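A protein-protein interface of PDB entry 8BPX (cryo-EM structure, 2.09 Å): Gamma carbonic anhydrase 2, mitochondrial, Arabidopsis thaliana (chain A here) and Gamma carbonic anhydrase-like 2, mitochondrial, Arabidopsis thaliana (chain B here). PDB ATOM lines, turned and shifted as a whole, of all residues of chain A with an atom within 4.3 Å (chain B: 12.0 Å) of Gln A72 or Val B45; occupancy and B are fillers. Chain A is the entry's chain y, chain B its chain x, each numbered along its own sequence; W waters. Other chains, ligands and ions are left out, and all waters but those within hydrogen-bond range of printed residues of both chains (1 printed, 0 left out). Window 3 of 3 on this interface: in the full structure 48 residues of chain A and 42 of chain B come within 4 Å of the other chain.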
ATOM      1  N   LEU A  54      24.477 -24.464  23.658  1.00  0.00           N
ATOM      2  CA  LEU A  54      25.387 -25.279  24.453  1.00  0.00           C
ATOM      3  C   LEU A  54      26.563 -25.658  23.561  1.00  0.00           C
ATOM      4  O   LEU A  54      26.431 -26.521  22.686  1.00  0.00           O
ATOM      5  CB  LEU A  54      24.677 -26.517  24.997  1.00  0.00           C
ATOM      6  CG  LEU A  54      25.477 -27.351  26.003  1.00  0.00           C
ATOM      7  CD1 LEU A  54      25.955 -26.478  27.145  1.00  0.00           C
ATOM      8  CD2 LEU A  54      24.650 -28.516  26.522  1.00  0.00           C
ATOM      9  N   VAL A  55      27.705 -25.015  23.779  1.00  0.00           N
ATOM     10  CA  VAL A  55      28.886 -25.189  22.943  1.00  0.00           C
ATOM     11  C   VAL A  55      30.013 -25.736  23.804  1.00  0.00           C
ATOM     12  O   VAL A  55      30.342 -25.159  24.844  1.00  0.00           O
ATOM     13  CB  VAL A  55      29.304 -23.870  22.269  1.00  0.00           C
ATOM     14  CG1 VAL A  55      30.458 -24.107  21.312  1.00  0.00           C
ATOM     15  CG2 VAL A  55      28.122 -23.250  21.546  1.00  0.00           C
ATOM     16  N   ASP A  56      30.610 -26.837  23.360  1.00  0.00           N
ATOM     17  CA  ASP A  56      31.691 -27.450  24.111  1.00  0.00           C
ATOM     18  C   ASP A  56      32.903 -26.525  24.171  1.00  0.00           C
ATOM     19  O   ASP A  56      33.096 -25.646  23.325  1.00  0.00           O
ATOM     20  CB  ASP A  56      32.084 -28.792  23.493  1.00  0.00           C
ATOM     21  CG  ASP A  56      32.945 -29.624  24.417  1.00  0.00           C
ATOM     22  OD1 ASP A  56      32.381 -30.340  25.272  1.00  0.00           O
ATOM     23  OD2 ASP A  56      34.187 -29.550  24.301  1.00  0.00           O
ATOM     24  N   VAL A  71      20.907 -24.594  20.324  1.00  0.00           N
ATOM     25  CA  VAL A  71      21.921 -25.236  19.496  1.00  0.00           C
ATOM     26  C   VAL A  71      22.915 -25.936  20.409  1.00  0.00           C
ATOM     27  O   VAL A  71      23.393 -25.342  21.382  1.00  0.00           O
ATOM     28  CB  VAL A  71      22.650 -24.221  18.590  1.00  0.00           C
ATOM     29  CG1 VAL A  71      23.713 -24.915  17.749  1.00  0.00           C
ATOM     30  CG2 VAL A  71      21.662 -23.478  17.710  1.00  0.00           C
ATOM     31  N   GLN A  72      23.238 -27.185  20.091  1.00  0.00           N
ATOM     32  CA  GLN A  72      24.239 -27.951  20.819  1.00  0.00           C
ATOM     33  C   GLN A  72      25.351 -28.371  19.870  1.00  0.00           C
ATOM     34  O   GLN A  72      25.085 -28.928  18.801  1.00  0.00           O
ATOM     35  CB  GLN A  72      23.617 -29.179  21.480  1.00  0.00           C
ATOM     36  CG  GLN A  72      24.515 -29.830  22.502  1.00  0.00           C
ATOM     37  CD  GLN A  72      24.012 -31.190  22.924  1.00  0.00           C
ATOM     38  OE1 GLN A  72      24.358 -32.204  22.322  1.00  0.00           O
ATOM     39  NE2 GLN A  72      23.192 -31.221  23.965  1.00  0.00           N
ATOM     40  N   ILE A  73      26.596 -28.114  20.266  1.00  0.00           N
ATOM     41  CA  ILE A  73      27.763 -28.403  19.441  1.00  0.00           C
ATOM     42  C   ILE A  73      28.760 -29.207  20.266  1.00  0.00           C
ATOM     43  O   ILE A  73      29.177 -28.769  21.343  1.00  0.00           O
ATOM     44  CB  ILE A  73      28.414 -27.115  18.900  1.00  0.00           C
ATOM     45  CG1 ILE A  73      27.406 -26.304  18.083  1.00  0.00           C
ATOM     46  CG2 ILE A  73      29.623 -27.451  18.057  1.00  0.00           C
ATOM     47  CD1 ILE A  73      27.804 -24.860  17.888  1.00  0.00           C
ATOM     48  N   GLY A  74      29.158 -30.373  19.747  1.00  0.00           N
ATOM     49  CA  GLY A  74      29.977 -31.300  20.496  1.00  0.00           C
ATOM     50  C   GLY A  74      31.479 -31.063  20.378  1.00  0.00           C
ATOM     51  O   GLY A  74      31.949 -30.197  19.644  1.00  0.00           O
ATOM     52  N   ILE A  92      18.779 -27.672  17.207  1.00  0.00           N
ATOM     53  CA  ILE A  92      19.870 -28.055  16.317  1.00  0.00           C
ATOM     54  C   ILE A  92      20.935 -28.747  17.152  1.00  0.00           C
ATOM     55  O   ILE A  92      21.392 -28.198  18.160  1.00  0.00           O
ATOM     56  CB  ILE A  92      20.477 -26.847  15.578  1.00  0.00           C
ATOM     57  CG1 ILE A  92      19.422 -26.125  14.743  1.00  0.00           C
ATOM     58  CG2 ILE A  92      21.631 -27.300  14.698  1.00  0.00           C
ATOM     59  CD1 ILE A  92      19.987 -25.015  13.874  1.00  0.00           C
ATOM     60  N   SER A  93      21.339 -29.939  16.727  1.00  0.00           N
ATOM     61  CA  SER A  93      22.346 -30.716  17.438  1.00  0.00           C
ATOM     62  C   SER A  93      23.473 -31.077  16.484  1.00  0.00           C
ATOM     63  O   SER A  93      23.228 -31.631  15.408  1.00  0.00           O
ATOM     64  CB  SER A  93      21.737 -31.979  18.048  1.00  0.00           C
ATOM     65  OG  SER A  93      21.301 -31.740  19.372  1.00  0.00           O
ATOM     66  N   VAL A  94      24.701 -30.765  16.884  1.00  0.00           N
ATOM     67  CA  VAL A  94      25.895 -31.064  16.107  1.00  0.00           C
ATOM     68  C   VAL A  94      26.780 -31.982  16.935  1.00  0.00           C
ATOM     69  O   VAL A  94      27.118 -31.659  18.080  1.00  0.00           O
ATOM     70  CB  VAL A  94      26.653 -29.787  15.708  1.00  0.00           C
ATOM     71  CG1 VAL A  94      27.921 -30.139  14.944  1.00  0.00           C
ATOM     72  CG2 VAL A  94      25.754 -28.875  14.885  1.00  0.00           C
ATOM     73  N   GLN B  44      29.857 -36.094  26.245  1.00  0.00           N
ATOM     74  CA  GLN B  44      29.369 -34.966  27.030  1.00  0.00           C
ATOM     75  C   GLN B  44      29.783 -33.642  26.401  1.00  0.00           C
ATOM     76  O   GLN B  44      30.877 -33.522  25.848  1.00  0.00           O
ATOM     77  CB  GLN B  44      29.888 -35.045  28.467  1.00  0.00           C
ATOM     78  CG  GLN B  44      29.167 -34.124  29.438  1.00  0.00           C
ATOM     79  CD  GLN B  44      29.992 -33.814  30.671  1.00  0.00           C
ATOM     80  OE1 GLN B  44      31.214 -33.679  30.599  1.00  0.00           O
ATOM     81  NE2 GLN B  44      29.327 -33.698  31.814  1.00  0.00           N
ATOM     82  N   VAL B  45      28.905 -32.649  26.486  1.00  0.00           N
ATOM     83  CA  VAL B  45      29.172 -31.313  25.970  1.00  0.00           C
ATOM     84  C   VAL B  45      29.454 -30.423  27.174  1.00  0.00           C
ATOM     85  O   VAL B  45      28.534 -29.914  27.820  1.00  0.00           O
ATOM     86  CB  VAL B  45      28.011 -30.784  25.124  1.00  0.00           C
ATOM     87  CG1 VAL B  45      28.282 -29.357  24.678  1.00  0.00           C
ATOM     88  CG2 VAL B  45      27.790 -31.678  23.920  1.00  0.00           C
ATOM     89  N   THR B  46      30.735 -30.243  27.488  1.00  0.00           N
ATOM     90  CA  THR B  46      31.128 -29.428  28.625  1.00  0.00           C
ATOM     91  C   THR B  46      31.572 -28.056  28.144  1.00  0.00           C
ATOM     92  O   THR B  46      32.649 -27.936  27.541  1.00  0.00           O
ATOM     93  CB  THR B  46      32.240 -30.110  29.426  1.00  0.00           C
ATOM     94  OG1 THR B  46      32.463 -29.399  30.648  1.00  0.00           O
ATOM     95  CG2 THR B  46      33.534 -30.206  28.619  1.00  0.00           C
ATOM     96  N   PRO B  47      30.789 -27.008  28.372  1.00  0.00           N
ATOM     97  CA  PRO B  47      31.143 -25.681  27.864  1.00  0.00           C
ATOM     98  C   PRO B  47      32.223 -25.016  28.706  1.00  0.00           C
ATOM     99  O   PRO B  47      32.596 -25.482  29.781  1.00  0.00           O
ATOM    100  CB  PRO B  47      29.824 -24.908  27.955  1.00  0.00           C
ATOM    101  CG  PRO B  47      29.084 -25.573  29.048  1.00  0.00           C
ATOM    102  CD  PRO B  47      29.463 -27.024  29.010  1.00  0.00           C
ATOM    103  N   SER B  48      32.720 -23.899  28.183  1.00  0.00           N
ATOM    104  CA  SER B  48      33.669 -23.044  28.872  1.00  0.00           C
ATOM    105  C   SER B  48      32.995 -21.752  29.294  1.00  0.00           C
ATOM    106  O   SER B  48      32.346 -21.099  28.465  1.00  0.00           O
ATOM    107  CB  SER B  48      34.871 -22.729  27.978  1.00  0.00           C
ATOM    108  OG  SER B  48      34.525 -21.818  26.953  1.00  0.00           O
ATOM    109  N   PRO B  49      33.124 -21.347  30.560  1.00  0.00           N
ATOM    110  CA  PRO B  49      32.531 -20.069  30.984  1.00  0.00           C
ATOM    111  C   PRO B  49      33.158 -18.857  30.321  1.00  0.00           C
ATOM    112  O   PRO B  49      32.507 -17.808  30.250  1.00  0.00           O
ATOM    113  CB  PRO B  49      32.764 -20.053  32.504  1.00  0.00           C
ATOM    114  CG  PRO B  49      33.213 -21.448  32.865  1.00  0.00           C
ATOM    115  CD  PRO B  49      33.882 -21.987  31.644  1.00  0.00           C
ATOM    116  N   ARG B  51      34.198 -18.421  27.114  1.00  0.00           N
ATOM    117  CA  ARG B  51      34.087 -18.250  25.670  1.00  0.00           C
ATOM    118  C   ARG B  51      33.355 -16.951  25.347  1.00  0.00           C
ATOM    119  O   ARG B  51      32.347 -16.613  25.973  1.00  0.00           O
ATOM    120  CB  ARG B  51      33.374 -19.441  25.023  1.00  0.00           C
ATOM    121  CG  ARG B  51      32.625 -19.098  23.731  1.00  0.00           C
ATOM    122  CD  ARG B  51      31.785 -20.250  23.199  1.00  0.00           C
ATOM    123  NE  ARG B  51      32.512 -21.513  23.133  1.00  0.00           N
ATOM    124  CZ  ARG B  51      33.387 -21.833  22.188  1.00  0.00           C
ATOM    125  NH1 ARG B  51      33.682 -20.998  21.206  1.00  0.00           N
ATOM    126  NH2 ARG B  51      33.975 -23.026  22.224  1.00  0.00           N
ATOM    127  N   LYS B  53      30.977 -14.475  23.846  1.00  0.00           N
ATOM    128  CA  LYS B  53      29.675 -14.436  23.195  1.00  0.00           C
ATOM    129  C   LYS B  53      29.539 -13.233  22.270  1.00  0.00           C
ATOM    130  O   LYS B  53      29.012 -13.358  21.162  1.00  0.00           O
ATOM    131  CB  LYS B  53      28.566 -14.412  24.247  1.00  0.00           C
ATOM    132  CG  LYS B  53      28.407 -15.718  25.002  1.00  0.00           C
ATOM    133  CD  LYS B  53      27.154 -15.709  25.846  1.00  0.00           C
ATOM    134  CE  LYS B  53      25.938 -15.364  25.009  1.00  0.00           C
ATOM    135  NZ  LYS B  53      25.148 -16.569  24.661  1.00  0.00           N
HETATM  136  O   HOH W   1      32.011 -23.221  25.513  1.00  0.00           O
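The backbone NH (N) of Thr B46 lies within hydrogen-bond range of the side-chain carboxylate (OD1) of Asp A56. NH2 of Arg B51 sits at hydrogen-bond distance from O of Asp A56, 3.0 Å away.
N of Arg B51 lies close to OG of Ser B48 (3.4 Å). The backbone NH (N) of Leu A54 sits at hydrogen-bond distance from the backbone carbonyl oxygen (O) of Val A71, 2.7 Å away. O of Leu A54 sits at hydrogen-bond distance from N of Ile A73, 2.9 Å away. N of Asp A56 lies within hydrogen-bond range of O of Ile A73. N of Gln A72 sits at hydrogen-bond distance from O of Ile A92 (2.9 Å). The backbone NH (N) of Val A94 sits at hydrogen-bond distance from the backbone carbonyl oxygen (O) of Gln A72 (2.7 Å).
Among the printed residues, merely in contact across the chains: Val A55 with Pro B47 (3.2 Å), Asp A56 with Val B45 (3.4 Å), Ile A73 with Val B45 (3.5 Å), Asp A56 with Gln B44 (3.6 Å), Leu A54 with Val B45 (3.7 Å), Leu A54 with Pro B47 (3.8 Å), Val A55 with Arg B51 (3.8 Å) and Gln A72 with Val B45 (3.8 Å).
Gln A72 touches just one residue of chain B: Val B45 (3.8 Å). Of chain A, only Leu A54, Asp A56, Gln A72 and Ile A73 come within 4 Å of Val B45. Of chain B, only Pro B47 and Arg B51 come within 4 Å of Val A55. Asp A56 touches just these residues of chain B: Gln B44 (3.6 Å), Val B45 (3.4 Å), Thr B46 (2.8 Å) and Arg B51 (3.0 Å). Ile A73 touches just one residue of chain B: Val B45 (3.5 Å). No residue of chain B comes within 4 Å of Gly A74. No residue of chain B comes within 4 Å of Ile A92. No residue of chain B comes within 4 Å of Ser A93. No residue of chain B comes within 4 Å of Val A94. Of the printed residues of chain A, Arg B51 touches Val A55 and Asp A56. Of the printed residues of chain A, Pro B47 touches Leu A54 (3.8 Å) and Val A55 (3.2 Å). Of the printed residues of chain A, Gln B44 touches Asp A56. The nearest residue of chain B that does not touch Gln A72 is Gln B44 (6.9 Å).
Of the 10 printed residues of chain A, 5 touch a printed residue of chain B. Printed residues of chain A that touch a printed residue of chain B: Leu A54, Val A55, Asp A56, Gln A72 and Ile A73. Hydrophobic or aromatic side chains of chain A within 4 Å of the printed part of chain B: Leu A54 and Val A55. Of the 8 printed residues of chain B, 5 touch a printed residue of chain A. Among the printed residues, no Asp or Glu carboxylate lies within 4 Å of a Lys or Arg side-chain nitrogen of the other chain.
Water W1 lies within hydrogen-bond range of the backbone carbonyl oxygen (O) of Val A55 (2.6 Å), the backbone NH (N) of Ser B48 (2.8 Å), the guanidinium group (NE) of Arg B51 (3.0 Å) and the backbone carbonyl oxygen (O) of Asp A56 (3.4 Å).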
